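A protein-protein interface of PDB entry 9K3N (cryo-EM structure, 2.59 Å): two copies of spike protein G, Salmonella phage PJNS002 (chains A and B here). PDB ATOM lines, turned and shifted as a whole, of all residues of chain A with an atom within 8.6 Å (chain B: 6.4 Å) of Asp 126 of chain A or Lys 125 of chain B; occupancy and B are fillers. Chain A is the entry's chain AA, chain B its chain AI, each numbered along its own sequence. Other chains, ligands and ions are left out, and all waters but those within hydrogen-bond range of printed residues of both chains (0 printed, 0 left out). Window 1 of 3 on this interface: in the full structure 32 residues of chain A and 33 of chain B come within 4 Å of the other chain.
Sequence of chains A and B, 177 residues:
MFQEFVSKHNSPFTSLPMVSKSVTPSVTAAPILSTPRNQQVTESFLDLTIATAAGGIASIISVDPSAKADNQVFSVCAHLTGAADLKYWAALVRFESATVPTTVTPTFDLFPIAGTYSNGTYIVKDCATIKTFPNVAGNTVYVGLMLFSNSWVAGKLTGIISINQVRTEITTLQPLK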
ATOM      1  N   LYS A   8      -2.695 -31.558  17.722  1.00  0.00           N
ATOM      2  CA  LYS A   8      -1.959 -30.647  16.863  1.00  0.00           C
ATOM      3  C   LYS A   8      -0.541 -31.168  16.663  1.00  0.00           C
ATOM      4  O   LYS A   8       0.039 -31.794  17.555  1.00  0.00           O
ATOM      5  CB  LYS A   8      -1.929 -29.238  17.465  1.00  0.00           C
ATOM      6  CG  LYS A   8      -3.307 -28.613  17.627  1.00  0.00           C
ATOM      7  CD  LYS A   8      -3.471 -27.950  18.985  1.00  0.00           C
ATOM      8  CE  LYS A   8      -2.515 -26.785  19.160  1.00  0.00           C
ATOM      9  NZ  LYS A   8      -2.665 -26.147  20.497  1.00  0.00           N
ATOM     10  N   HIS A   9       0.008 -30.913  15.478  1.00  0.00           N
ATOM     11  CA  HIS A   9       1.368 -31.309  15.117  1.00  0.00           C
ATOM     12  C   HIS A   9       1.559 -32.827  15.203  1.00  0.00           C
ATOM     13  O   HIS A   9       2.241 -33.356  16.084  1.00  0.00           O
ATOM     14  CB  HIS A   9       2.418 -30.592  15.971  1.00  0.00           C
ATOM     15  CG  HIS A   9       3.823 -30.938  15.592  1.00  0.00           C
ATOM     16  ND1 HIS A   9       4.415 -30.481  14.435  1.00  0.00           N
ATOM     17  CD2 HIS A   9       4.742 -31.729  16.198  1.00  0.00           C
ATOM     18  CE1 HIS A   9       5.644 -30.958  14.354  1.00  0.00           C
ATOM     19  NE2 HIS A   9       5.867 -31.717  15.411  1.00  0.00           N
ATOM     20  N   ASN A  10       0.897 -33.524  14.286  1.00  0.00           N
ATOM     21  CA  ASN A  10       1.293 -34.896  14.008  1.00  0.00           C
ATOM     22  C   ASN A  10       2.745 -34.918  13.543  1.00  0.00           C
ATOM     23  O   ASN A  10       3.154 -34.123  12.691  1.00  0.00           O
ATOM     24  CB  ASN A  10       0.377 -35.517  12.956  1.00  0.00           C
ATOM     25  CG  ASN A  10      -1.041 -35.695  13.453  1.00  0.00           C
ATOM     26  OD1 ASN A  10      -1.359 -36.686  14.107  1.00  0.00           O
ATOM     27  ND2 ASN A  10      -1.902 -34.731  13.147  1.00  0.00           N
ATOM     28  N   VAL A  73      -2.095 -25.147   6.850  1.00  0.00           N
ATOM     29  CA  VAL A  73      -1.771 -25.119   8.273  1.00  0.00           C
ATOM     30  C   VAL A  73      -0.373 -25.682   8.487  1.00  0.00           C
ATOM     31  O   VAL A  73      -0.010 -26.717   7.915  1.00  0.00           O
ATOM     32  CB  VAL A  73      -2.815 -25.906   9.091  1.00  0.00           C
ATOM     33  CG1 VAL A  73      -2.446 -25.913  10.568  1.00  0.00           C
ATOM     34  CG2 VAL A  73      -4.202 -25.320   8.889  1.00  0.00           C
ATOM     35  N   PHE A  74       0.418 -24.991   9.309  1.00  0.00           N
ATOM     36  CA  PHE A  74       1.752 -25.424   9.697  1.00  0.00           C
ATOM     37  C   PHE A  74       1.821 -25.527  11.216  1.00  0.00           C
ATOM     38  O   PHE A  74       1.308 -24.659  11.929  1.00  0.00           O
ATOM     39  CB  PHE A  74       2.826 -24.455   9.189  1.00  0.00           C
ATOM     40  CG  PHE A  74       2.948 -24.411   7.693  1.00  0.00           C
ATOM     41  CD1 PHE A  74       2.070 -23.656   6.932  1.00  0.00           C
ATOM     42  CD2 PHE A  74       3.949 -25.118   7.046  1.00  0.00           C
ATOM     43  CE1 PHE A  74       2.182 -23.614   5.556  1.00  0.00           C
ATOM     44  CE2 PHE A  74       4.066 -25.077   5.669  1.00  0.00           C
ATOM     45  CZ  PHE A  74       3.180 -24.325   4.925  1.00  0.00           C
ATOM     46  N   SER A  75       2.463 -26.583  11.709  1.00  0.00           N
ATOM     47  CA  SER A  75       2.531 -26.865  13.134  1.00  0.00           C
ATOM     48  C   SER A  75       3.981 -27.011  13.583  1.00  0.00           C
ATOM     49  O   SER A  75       4.893 -27.205  12.774  1.00  0.00           O
ATOM     50  CB  SER A  75       1.733 -28.128  13.478  1.00  0.00           C
ATOM     51  OG  SER A  75       2.197 -29.242  12.734  1.00  0.00           O
ATOM     52  N   VAL A  76       4.186 -26.921  14.897  1.00  0.00           N
ATOM     53  CA  VAL A  76       5.522 -26.927  15.481  1.00  0.00           C
ATOM     54  C   VAL A  76       5.447 -27.515  16.885  1.00  0.00           C
ATOM     55  O   VAL A  76       4.449 -27.353  17.594  1.00  0.00           O
ATOM     56  CB  VAL A  76       6.127 -25.501  15.496  1.00  0.00           C
ATOM     57  CG1 VAL A  76       5.218 -24.542  16.250  1.00  0.00           C
ATOM     58  CG2 VAL A  76       7.528 -25.501  16.097  1.00  0.00           C
ATOM     59  N   CYS A  77       6.510 -28.216  17.277  1.00  0.00           N
ATOM     60  CA  CYS A  77       6.666 -28.710  18.640  1.00  0.00           C
ATOM     61  C   CYS A  77       8.151 -28.754  18.966  1.00  0.00           C
ATOM     62  O   CYS A  77       8.929 -29.359  18.221  1.00  0.00           O
ATOM     63  CB  CYS A  77       6.037 -30.096  18.811  1.00  0.00           C
ATOM     64  SG  CYS A  77       6.089 -30.750  20.494  1.00  0.00           S
ATOM     65  N   ALA A  78       8.559 -28.077  20.033  1.00  0.00           N
ATOM     66  CA  ALA A  78       9.981 -28.012  20.355  1.00  0.00           C
ATOM     67  C   ALA A  78      10.234 -27.853  21.841  1.00  0.00           C
ATOM     68  O   ALA A  78       9.569 -27.062  22.510  1.00  0.00           O
ATOM     69  CB  ALA A  78      10.640 -26.872  19.587  1.00  0.00           C
ATOM     70  N   LEU A  92       7.137 -18.021  14.386  1.00  0.00           N
ATOM     71  CA  LEU A  92       7.197 -18.605  13.053  1.00  0.00           C
ATOM     72  C   LEU A  92       7.663 -17.569  12.036  1.00  0.00           C
ATOM     73  O   LEU A  92       7.480 -16.364  12.215  1.00  0.00           O
ATOM     74  CB  LEU A  92       5.835 -19.165  12.640  1.00  0.00           C
ATOM     75  CG  LEU A  92       5.376 -20.457  13.319  1.00  0.00           C
ATOM     76  CD1 LEU A  92       4.036 -20.911  12.759  1.00  0.00           C
ATOM     77  CD2 LEU A  92       6.420 -21.550  13.170  1.00  0.00           C
ATOM     78  N   PHE A 111       4.813 -14.786  12.552  1.00  0.00           N
ATOM     79  CA  PHE A 111       3.510 -15.204  13.031  1.00  0.00           C
ATOM     80  C   PHE A 111       3.590 -15.519  14.519  1.00  0.00           C
ATOM     81  O   PHE A 111       4.461 -16.298  14.934  1.00  0.00           O
ATOM     82  CB  PHE A 111       3.008 -16.433  12.255  1.00  0.00           C
ATOM     83  CG  PHE A 111       2.765 -16.169  10.798  1.00  0.00           C
ATOM     84  CD1 PHE A 111       3.806 -16.233   9.884  1.00  0.00           C
ATOM     85  CD2 PHE A 111       1.497 -15.854  10.338  1.00  0.00           C
ATOM     86  CE1 PHE A 111       3.586 -15.986   8.541  1.00  0.00           C
ATOM     87  CE2 PHE A 111       1.271 -15.608   8.997  1.00  0.00           C
ATOM     88  CZ  PHE A 111       2.318 -15.674   8.098  1.00  0.00           C
ATOM     89  N   PRO A 112       2.726 -14.934  15.347  1.00  0.00           N
ATOM     90  CA  PRO A 112       2.808 -15.178  16.793  1.00  0.00           C
ATOM     91  C   PRO A 112       2.587 -16.643  17.138  1.00  0.00           C
ATOM     92  O   PRO A 112       1.767 -17.332  16.527  1.00  0.00           O
ATOM     93  CB  PRO A 112       1.694 -14.294  17.365  1.00  0.00           C
ATOM     94  CG  PRO A 112       1.446 -13.261  16.318  1.00  0.00           C
ATOM     95  CD  PRO A 112       1.686 -13.949  15.011  1.00  0.00           C
ATOM     96  N   ILE A 113       3.329 -17.112  18.139  1.00  0.00           N
ATOM     97  CA  ILE A 113       3.252 -18.488  18.618  1.00  0.00           C
ATOM     98  C   ILE A 113       3.300 -18.460  20.139  1.00  0.00           C
ATOM     99  O   ILE A 113       4.151 -17.779  20.724  1.00  0.00           O
ATOM    100  CB  ILE A 113       4.392 -19.350  18.041  1.00  0.00           C
ATOM    101  CG1 ILE A 113       4.064 -19.779  16.609  1.00  0.00           C
ATOM    102  CG2 ILE A 113       4.650 -20.560  18.904  1.00  0.00           C
ATOM    103  CD1 ILE A 113       2.844 -20.664  16.497  1.00  0.00           C
ATOM    104  N   ALA A 114       2.392 -19.192  20.781  1.00  0.00           N
ATOM    105  CA  ALA A 114       2.232 -19.164  22.229  1.00  0.00           C
ATOM    106  C   ALA A 114       2.780 -20.453  22.832  1.00  0.00           C
ATOM    107  O   ALA A 114       2.250 -21.538  22.573  1.00  0.00           O
ATOM    108  CB  ALA A 114       0.764 -18.978  22.611  1.00  0.00           C
ATOM    109  N   GLY A 115       3.825 -20.325  23.646  1.00  0.00           N
ATOM    110  CA  GLY A 115       4.424 -21.465  24.310  1.00  0.00           C
ATOM    111  C   GLY A 115       4.637 -21.243  25.795  1.00  0.00           C
ATOM    112  O   GLY A 115       3.826 -20.583  26.452  1.00  0.00           O
ATOM    113  N   TYR A 122      12.184 -23.573  26.623  1.00  0.00           N
ATOM    114  CA  TYR A 122      11.039 -23.195  25.808  1.00  0.00           C
ATOM    115  C   TYR A 122      10.340 -24.445  25.295  1.00  0.00           C
ATOM    116  O   TYR A 122      10.980 -25.321  24.702  1.00  0.00           O
ATOM    117  CB  TYR A 122      11.468 -22.305  24.637  1.00  0.00           C
ATOM    118  CG  TYR A 122      10.314 -21.804  23.803  1.00  0.00           C
ATOM    119  CD1 TYR A 122       9.438 -20.848  24.301  1.00  0.00           C
ATOM    120  CD2 TYR A 122      10.103 -22.279  22.515  1.00  0.00           C
ATOM    121  CE1 TYR A 122       8.382 -20.386  23.544  1.00  0.00           C
ATOM    122  CE2 TYR A 122       9.050 -21.818  21.750  1.00  0.00           C
ATOM    123  CZ  TYR A 122       8.193 -20.873  22.268  1.00  0.00           C
ATOM    124  OH  TYR A 122       7.140 -20.414  21.511  1.00  0.00           O
ATOM    125  N   ILE A 123       9.032 -24.522  25.526  1.00  0.00           N
ATOM    126  CA  ILE A 123       8.204 -25.639  25.084  1.00  0.00           C
ATOM    127  C   ILE A 123       6.957 -25.069  24.423  1.00  0.00           C
ATOM    128  O   ILE A 123       6.357 -24.117  24.931  1.00  0.00           O
ATOM    129  CB  ILE A 123       7.825 -26.568  26.259  1.00  0.00           C
ATOM    130  CG1 ILE A 123       9.076 -27.007  27.025  1.00  0.00           C
ATOM    131  CG2 ILE A 123       7.061 -27.784  25.761  1.00  0.00           C
ATOM    132  CD1 ILE A 123       8.778 -27.823  28.264  1.00  0.00           C
ATOM    133  N   VAL A 124       6.566 -25.648  23.287  1.00  0.00           N
ATOM    134  CA  VAL A 124       5.416 -25.153  22.536  1.00  0.00           C
ATOM    135  C   VAL A 124       4.871 -26.286  21.679  1.00  0.00           C
ATOM    136  O   VAL A 124       5.615 -27.162  21.235  1.00  0.00           O
ATOM    137  CB  VAL A 124       5.799 -23.915  21.684  1.00  0.00           C
ATOM    138  CG1 VAL A 124       6.803 -24.293  20.603  1.00  0.00           C
ATOM    139  CG2 VAL A 124       4.560 -23.285  21.080  1.00  0.00           C
ATOM    140  N   LYS A 125       3.554 -26.281  21.472  1.00  0.00           N
ATOM    141  CA  LYS A 125       2.874 -27.243  20.607  1.00  0.00           C
ATOM    142  C   LYS A 125       1.773 -26.543  19.809  1.00  0.00           C
ATOM    143  O   LYS A 125       0.643 -27.021  19.710  1.00  0.00           O
ATOM    144  CB  LYS A 125       2.318 -28.405  21.426  1.00  0.00           C
ATOM    145  CG  LYS A 125       1.994 -29.654  20.618  1.00  0.00           C
ATOM    146  CD  LYS A 125       1.301 -30.694  21.484  1.00  0.00           C
ATOM    147  CE  LYS A 125       0.969 -31.944  20.687  1.00  0.00           C
ATOM    148  NZ  LYS A 125       2.193 -32.609  20.166  1.00  0.00           N
ATOM    149  N   ASP A 126       2.090 -25.386  19.233  1.00  0.00           N
ATOM    150  CA  ASP A 126       1.097 -24.548  18.577  1.00  0.00           C
ATOM    151  C   ASP A 126       1.086 -24.789  17.066  1.00  0.00           C
ATOM    152  O   ASP A 126       1.897 -25.538  16.518  1.00  0.00           O
ATOM    153  CB  ASP A 126       1.359 -23.075  18.896  1.00  0.00           C
ATOM    154  CG  ASP A 126       0.085 -22.258  18.971  1.00  0.00           C
ATOM    155  OD1 ASP A 126      -0.931 -22.677  18.375  1.00  0.00           O
ATOM    156  OD2 ASP A 126       0.099 -21.196  19.626  1.00  0.00           O
ATOM    157  N   CYS A 127       0.138 -24.141  16.387  1.00  0.00           N
ATOM    158  CA  CYS A 127       0.005 -24.240  14.939  1.00  0.00           C
ATOM    159  C   CYS A 127      -0.649 -22.970  14.410  1.00  0.00           C
ATOM    160  O   CYS A 127      -1.284 -22.221  15.157  1.00  0.00           O
ATOM    161  CB  CYS A 127      -0.807 -25.475  14.529  1.00  0.00           C
ATOM    162  SG  CYS A 127      -2.470 -25.551  15.233  1.00  0.00           S
ATOM    163  N   ALA A 128      -0.490 -22.736  13.108  1.00  0.00           N
ATOM    164  CA  ALA A 128      -1.004 -21.524  12.483  1.00  0.00           C
ATOM    165  C   ALA A 128      -1.239 -21.767  10.998  1.00  0.00           C
ATOM    166  O   ALA A 128      -0.754 -22.742  10.420  1.00  0.00           O
ATOM    167  CB  ALA A 128      -0.050 -20.341  12.683  1.00  0.00           C
ATOM    168  N   THR A 129      -1.989 -20.853  10.385  1.00  0.00           N
ATOM    169  CA  THR A 129      -2.318 -20.904   8.965  1.00  0.00           C
ATOM    170  C   THR A 129      -1.501 -19.859   8.216  1.00  0.00           C
ATOM    171  O   THR A 129      -1.485 -18.686   8.603  1.00  0.00           O
ATOM    172  CB  THR A 129      -3.814 -20.662   8.740  1.00  0.00           C
ATOM    173  OG1 THR A 129      -4.567 -21.704   9.368  1.00  0.00           O
ATOM    174  CG2 THR A 129      -4.135 -20.640   7.254  1.00  0.00           C
ATOM    175  N   SER A 162      10.592 -29.917  15.769  1.00  0.00           N
ATOM    176  CA  SER A 162       9.875 -30.625  14.718  1.00  0.00           C
ATOM    177  C   SER A 162       8.899 -29.683  14.029  1.00  0.00           C
ATOM    178  O   SER A 162       8.189 -28.919  14.689  1.00  0.00           O
ATOM    179  CB  SER A 162       9.124 -31.839  15.282  1.00  0.00           C
ATOM    180  OG  SER A 162       8.464 -32.556  14.254  1.00  0.00           O
ATOM    181  N   ILE A 163       8.867 -29.745  12.698  1.00  0.00           N
ATOM    182  CA  ILE A 163       8.001 -28.907  11.874  1.00  0.00           C
ATOM    183  C   ILE A 163       7.198 -29.809  10.947  1.00  0.00           C
ATOM    184  O   ILE A 163       7.718 -30.813  10.443  1.00  0.00           O
ATOM    185  CB  ILE A 163       8.809 -27.878  11.055  1.00  0.00           C
ATOM    186  CG1 ILE A 163       9.797 -27.122  11.948  1.00  0.00           C
ATOM    187  CG2 ILE A 163       7.882 -26.896  10.358  1.00  0.00           C
ATOM    188  CD1 ILE A 163       9.136 -26.188  12.928  1.00  0.00           C
ATOM    189  N   ASN A 164       5.933 -29.461  10.723  1.00  0.00           N
ATOM    190  CA  ASN A 164       5.075 -30.226   9.832  1.00  0.00           C
ATOM    191  C   ASN A 164       4.235 -29.287   8.978  1.00  0.00           C
ATOM    192  O   ASN A 164       3.834 -28.209   9.422  1.00  0.00           O
ATOM    193  CB  ASN A 164       4.152 -31.178  10.609  1.00  0.00           C
ATOM    194  CG  ASN A 164       3.339 -32.076   9.697  1.00  0.00           C
ATOM    195  OD1 ASN A 164       3.809 -32.492   8.639  1.00  0.00           O
ATOM    196  ND2 ASN A 164       2.109 -32.372  10.097  1.00  0.00           N
ATOM    197  N   SER B   7      -8.960 -23.032  16.288  1.00  0.00           N
ATOM    198  CA  SER B   7      -7.980 -22.274  17.047  1.00  0.00           C
ATOM    199  C   SER B   7      -8.533 -20.898  17.375  1.00  0.00           C
ATOM    200  O   SER B   7      -9.497 -20.426  16.764  1.00  0.00           O
ATOM    201  CB  SER B   7      -6.657 -22.140  16.284  1.00  0.00           C
ATOM    202  OG  SER B   7      -5.764 -21.273  16.964  1.00  0.00           O
ATOM    203  N   LYS B   8      -7.913 -20.262  18.359  1.00  0.00           N
ATOM    204  CA  LYS B   8      -8.172 -18.874  18.698  1.00  0.00           C
ATOM    205  C   LYS B   8      -7.085 -17.993  18.096  1.00  0.00           C
ATOM    206  O   LYS B   8      -5.927 -18.402  17.974  1.00  0.00           O
ATOM    207  CB  LYS B   8      -8.229 -18.687  20.216  1.00  0.00           C
ATOM    208  CG  LYS B   8      -9.342 -19.478  20.889  1.00  0.00           C
ATOM    209  CD  LYS B   8      -8.855 -20.187  22.144  1.00  0.00           C
ATOM    210  CE  LYS B   8      -8.411 -19.200  23.207  1.00  0.00           C
ATOM    211  NZ  LYS B   8      -7.918 -19.895  24.429  1.00  0.00           N
ATOM    212  N   HIS B   9      -7.472 -16.778  17.709  1.00  0.00           N
ATOM    213  CA  HIS B   9      -6.563 -15.785  17.139  1.00  0.00           C
ATOM    214  C   HIS B   9      -5.896 -16.296  15.858  1.00  0.00           C
ATOM    215  O   HIS B   9      -4.700 -16.593  15.812  1.00  0.00           O
ATOM    216  CB  HIS B   9      -5.502 -15.334  18.148  1.00  0.00           C
ATOM    217  CG  HIS B   9      -4.586 -14.280  17.611  1.00  0.00           C
ATOM    218  ND1 HIS B   9      -4.989 -12.978  17.412  1.00  0.00           N
ATOM    219  CD2 HIS B   9      -3.300 -14.345  17.192  1.00  0.00           C
ATOM    220  CE1 HIS B   9      -3.983 -12.281  16.915  1.00  0.00           C
ATOM    221  NE2 HIS B   9      -2.947 -13.087  16.772  1.00  0.00           N
ATOM    222  N   ASN B  10      -6.716 -16.438  14.823  1.00  0.00           N
ATOM    223  CA  ASN B  10      -6.161 -16.524  13.479  1.00  0.00           C
ATOM    224  C   ASN B  10      -5.365 -15.260  13.180  1.00  0.00           C
ATOM    225  O   ASN B  10      -5.824 -14.143  13.432  1.00  0.00           O
ATOM    226  CB  ASN B  10      -7.273 -16.722  12.452  1.00  0.00           C
ATOM    227  CG  ASN B  10      -7.963 -18.062  12.594  1.00  0.00           C
ATOM    228  OD1 ASN B  10      -7.495 -19.072  12.069  1.00  0.00           O
ATOM    229  ND2 ASN B  10      -9.082 -18.081  13.309  1.00  0.00           N
ATOM    230  N   VAL B  76      -5.993 -12.048  20.739  1.00  0.00           N
ATOM    231  CA  VAL B  76      -4.658 -11.513  20.974  1.00  0.00           C
ATOM    232  C   VAL B  76      -3.687 -12.673  21.164  1.00  0.00           C
ATOM    233  O   VAL B  76      -4.047 -13.729  21.691  1.00  0.00           O
ATOM    234  CB  VAL B  76      -4.648 -10.563  22.199  1.00  0.00           C
ATOM    235  CG1 VAL B  76      -5.166 -11.281  23.437  1.00  0.00           C
ATOM    236  CG2 VAL B  76      -3.257  -9.993  22.446  1.00  0.00           C
ATOM    237  N   CYS B  77      -2.449 -12.471  20.712  1.00  0.00           N
ATOM    238  CA  CYS B  77      -1.361 -13.411  20.953  1.00  0.00           C
ATOM    239  C   CYS B  77      -0.058 -12.629  21.025  1.00  0.00           C
ATOM    240  O   CYS B  77       0.256 -11.870  20.103  1.00  0.00           O
ATOM    241  CB  CYS B  77      -1.289 -14.479  19.858  1.00  0.00           C
ATOM    242  SG  CYS B  77      -0.035 -15.754  20.123  1.00  0.00           S
ATOM    243  N   ALA B  78       0.670 -12.763  22.126  1.00  0.00           N
ATOM    244  CA  ALA B  78       1.890 -11.978  22.292  1.00  0.00           C
ATOM    245  C   ALA B  78       2.918 -12.678  23.159  1.00  0.00           C
ATOM    246  O   ALA B  78       2.583 -13.243  24.200  1.00  0.00           O
ATOM    247  CB  ALA B  78       1.557 -10.610  22.877  1.00  0.00           C
ATOM    248  N   ILE B 113      -7.748 -10.875  30.887  1.00  0.00           N
ATOM    249  CA  ILE B 113      -7.086 -11.758  29.934  1.00  0.00           C
ATOM    250  C   ILE B 113      -6.146 -12.670  30.711  1.00  0.00           C
ATOM    251  O   ILE B 113      -5.383 -12.199  31.561  1.00  0.00           O
ATOM    252  CB  ILE B 113      -6.324 -10.958  28.858  1.00  0.00           C
ATOM    253  CG1 ILE B 113      -7.290 -10.446  27.790  1.00  0.00           C
ATOM    254  CG2 ILE B 113      -5.238 -11.793  28.227  1.00  0.00           C
ATOM    255  CD1 ILE B 113      -7.979 -11.543  27.008  1.00  0.00           C
ATOM    256  N   ALA B 114      -6.201 -13.969  30.426  1.00  0.00           N
ATOM    257  CA  ALA B 114      -5.458 -14.976  31.173  1.00  0.00           C
ATOM    258  C   ALA B 114      -4.291 -15.482  30.335  1.00  0.00           C
ATOM    259  O   ALA B 114      -4.495 -16.096  29.284  1.00  0.00           O
ATOM    260  CB  ALA B 114      -6.369 -16.136  31.576  1.00  0.00           C
ATOM    261  N   GLY B 115      -3.072 -15.237  30.813  1.00  0.00           N
ATOM    262  CA  GLY B 115      -1.876 -15.689  30.131  1.00  0.00           C
ATOM    263  C   GLY B 115      -0.898 -16.391  31.052  1.00  0.00           C
ATOM    264  O   GLY B 115      -1.306 -17.096  31.979  1.00  0.00           O
ATOM    265  N   ILE B 123       3.203 -14.519  27.918  1.00  0.00           N
ATOM    266  CA  ILE B 123       2.677 -15.232  26.759  1.00  0.00           C
ATOM    267  C   ILE B 123       1.184 -15.439  26.969  1.00  0.00           C
ATOM    268  O   ILE B 123       0.749 -15.797  28.069  1.00  0.00           O
ATOM    269  CB  ILE B 123       3.395 -16.584  26.549  1.00  0.00           C
ATOM    270  CG1 ILE B 123       4.912 -16.390  26.503  1.00  0.00           C
ATOM    271  CG2 ILE B 123       2.913 -17.257  25.274  1.00  0.00           C
ATOM    272  CD1 ILE B 123       5.691 -17.683  26.420  1.00  0.00           C
ATOM    273  N   VAL B 124       0.395 -15.213  25.917  1.00  0.00           N
ATOM    274  CA  VAL B 124      -1.056 -15.329  26.016  1.00  0.00           C
ATOM    275  C   VAL B 124      -1.619 -15.597  24.628  1.00  0.00           C
ATOM    276  O   VAL B 124      -1.062 -15.153  23.621  1.00  0.00           O
ATOM    277  CB  VAL B 124      -1.673 -14.057  26.654  1.00  0.00           C
ATOM    278  CG1 VAL B 124      -1.464 -12.845  25.756  1.00  0.00           C
ATOM    279  CG2 VAL B 124      -3.146 -14.272  26.945  1.00  0.00           C
ATOM    280  N   LYS B 125      -2.713 -16.356  24.576  1.00  0.00           N
ATOM    281  CA  LYS B 125      -3.431 -16.642  23.336  1.00  0.00           C
ATOM    282  C   LYS B 125      -4.939 -16.616  23.587  1.00  0.00           C
ATOM    283  O   LYS B 125      -5.681 -17.502  23.164  1.00  0.00           O
ATOM    284  CB  LYS B 125      -2.985 -17.982  22.753  1.00  0.00           C
ATOM    285  CG  LYS B 125      -3.318 -18.177  21.281  1.00  0.00           C
ATOM    286  CD  LYS B 125      -2.983 -19.589  20.831  1.00  0.00           C
ATOM    287  CE  LYS B 125      -3.315 -19.797  19.364  1.00  0.00           C
ATOM    288  NZ  LYS B 125      -2.519 -18.898  18.485  1.00  0.00           N
ATOM    289  N   ASP B 126      -5.415 -15.593  24.294  1.00  0.00           N
ATOM    290  CA  ASP B 126      -6.801 -15.529  24.731  1.00  0.00           C
ATOM    291  C   ASP B 126      -7.641 -14.682  23.772  1.00  0.00           C
ATOM    292  O   ASP B 126      -7.138 -14.078  22.824  1.00  0.00           O
ATOM    293  CB  ASP B 126      -6.877 -14.984  26.159  1.00  0.00           C
ATOM    294  CG  ASP B 126      -8.027 -15.577  26.950  1.00  0.00           C
ATOM    295  OD1 ASP B 126      -9.001 -16.050  26.327  1.00  0.00           O
ATOM    296  OD2 ASP B 126      -7.955 -15.567  28.195  1.00  0.00           O
ATOM    297  N   CYS B 127      -8.949 -14.645  24.032  1.00  0.00           N
ATOM    298  CA  CYS B 127      -9.885 -13.865  23.233  1.00  0.00           C
ATOM    299  C   CYS B 127     -11.081 -13.485  24.097  1.00  0.00           C
ATOM    300  O   CYS B 127     -11.335 -14.093  25.139  1.00  0.00           O
ATOM    301  CB  CYS B 127     -10.342 -14.633  21.988  1.00  0.00           C
ATOM    302  SG  CYS B 127     -11.121 -16.229  22.329  1.00  0.00           S
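Of the 15 printed residues of chain B, 3 touch a printed residue of chain A. Printed residues of chain A that touch a printed residue of chain B: Pro 112, Ala 114, Gly 115 and Asp 126. Among the printed residues, 5 pairs touch across the chains. Among the printed residues, Asp or Glu carboxylates within 4 Å of a Lys or Arg side-chain nitrogen of the other chain: Asp 126 of chain A with Lys 125 of chain B.
Of the printed residues of chain B, Pro 112 of chain A touches Cys 77 (3.6 Å). Of the printed residues of chain B, Ala 114 of chain A touches Ile 123 and Lys 125. Of the printed residues of chain B, Gly 115 of chain A touches Ile 123. Asp 126 of chain A touches just one residue of chain B: Lys 125. Of the printed residues of chain A, Cys 77 of chain B touches Pro 112. Of the printed residues of chain A, Ile 123 of chain B touches Ala 114 (3.7 Å) and Gly 115 (3.4 Å). Of chain A, only Ala 114 (3.9 Å) and Asp 126 (3.7 Å) come within 4 Å of Lys 125 of chain B. Asp 126 of chain B touches none of the printed residues of chain A. Cys 127 of chain B touches none of the printed residues of chain A. The nearest residue of chain B that does not touch Asp 126 of chain A is Ser 7 of chain B (5.2 Å). The nearest residue of chain A that does not touch Lys 125 of chain B is Cys 127 of chain A (4.9 Å).
The side-chain amino group (NZ) of Lys 125 of chain B is in salt-bridge range of the side-chain carboxylate (OD2) of Asp 126 of chain A.
Among the printed residues, pairs that only touch across the chains: Pro 112 of chain A with Cys 77 of chain B, Ala 114 of chain A with Ile 123 of chain B, Ala 114 of chain A with Lys 125 of chain B and Gly 115 of chain A with Ile 123 of chain B.
N of Val 76 of chain A sits at hydrogen-bond distance from O of Asp 126 of chain A, 3.1 Å away. OD2 of Asp 126 of chain A is in hydrogen-bond range of N of Ala 114 of chain A, at 3.3 Å. O of Lys 8 of chain B lies close to NZ of Lys 125 of chain B. SG of Cys 77 of chain B sits close to O of Val 124 of chain B, at 3.7 Å.
Ala 114 of chain A touches Ile 123 of chain B, but with the chains exchanged Ile 123 of chain A does not touch Ala 114 of chain B (14.2 Å). Ala 114 of chain A touches Lys 125 of chain B, but with the chains exchanged Lys 125 of chain A does not touch Ala 114 of chain B (15.2 Å). Gly 115 of chain A touches Ile 123 of chain B, but with the chains exchanged Ile 123 of chain A does not touch Gly 115 of chain B (12.2 Å). Asp 126 of chain A touches Lys 125 of chain B, but with the chains exchanged Lys 125 of chain A does not touch Asp 126 of chain B (13.7 Å). Positions printed for both chains: 8, 9, 10, 76, 77, 78, 113, 114, 115, 123, 124, 125, 126 and 127. Of the 5 pairs that touch across the chains among the printed residues, none has its exchanged pair printed and touching as well.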
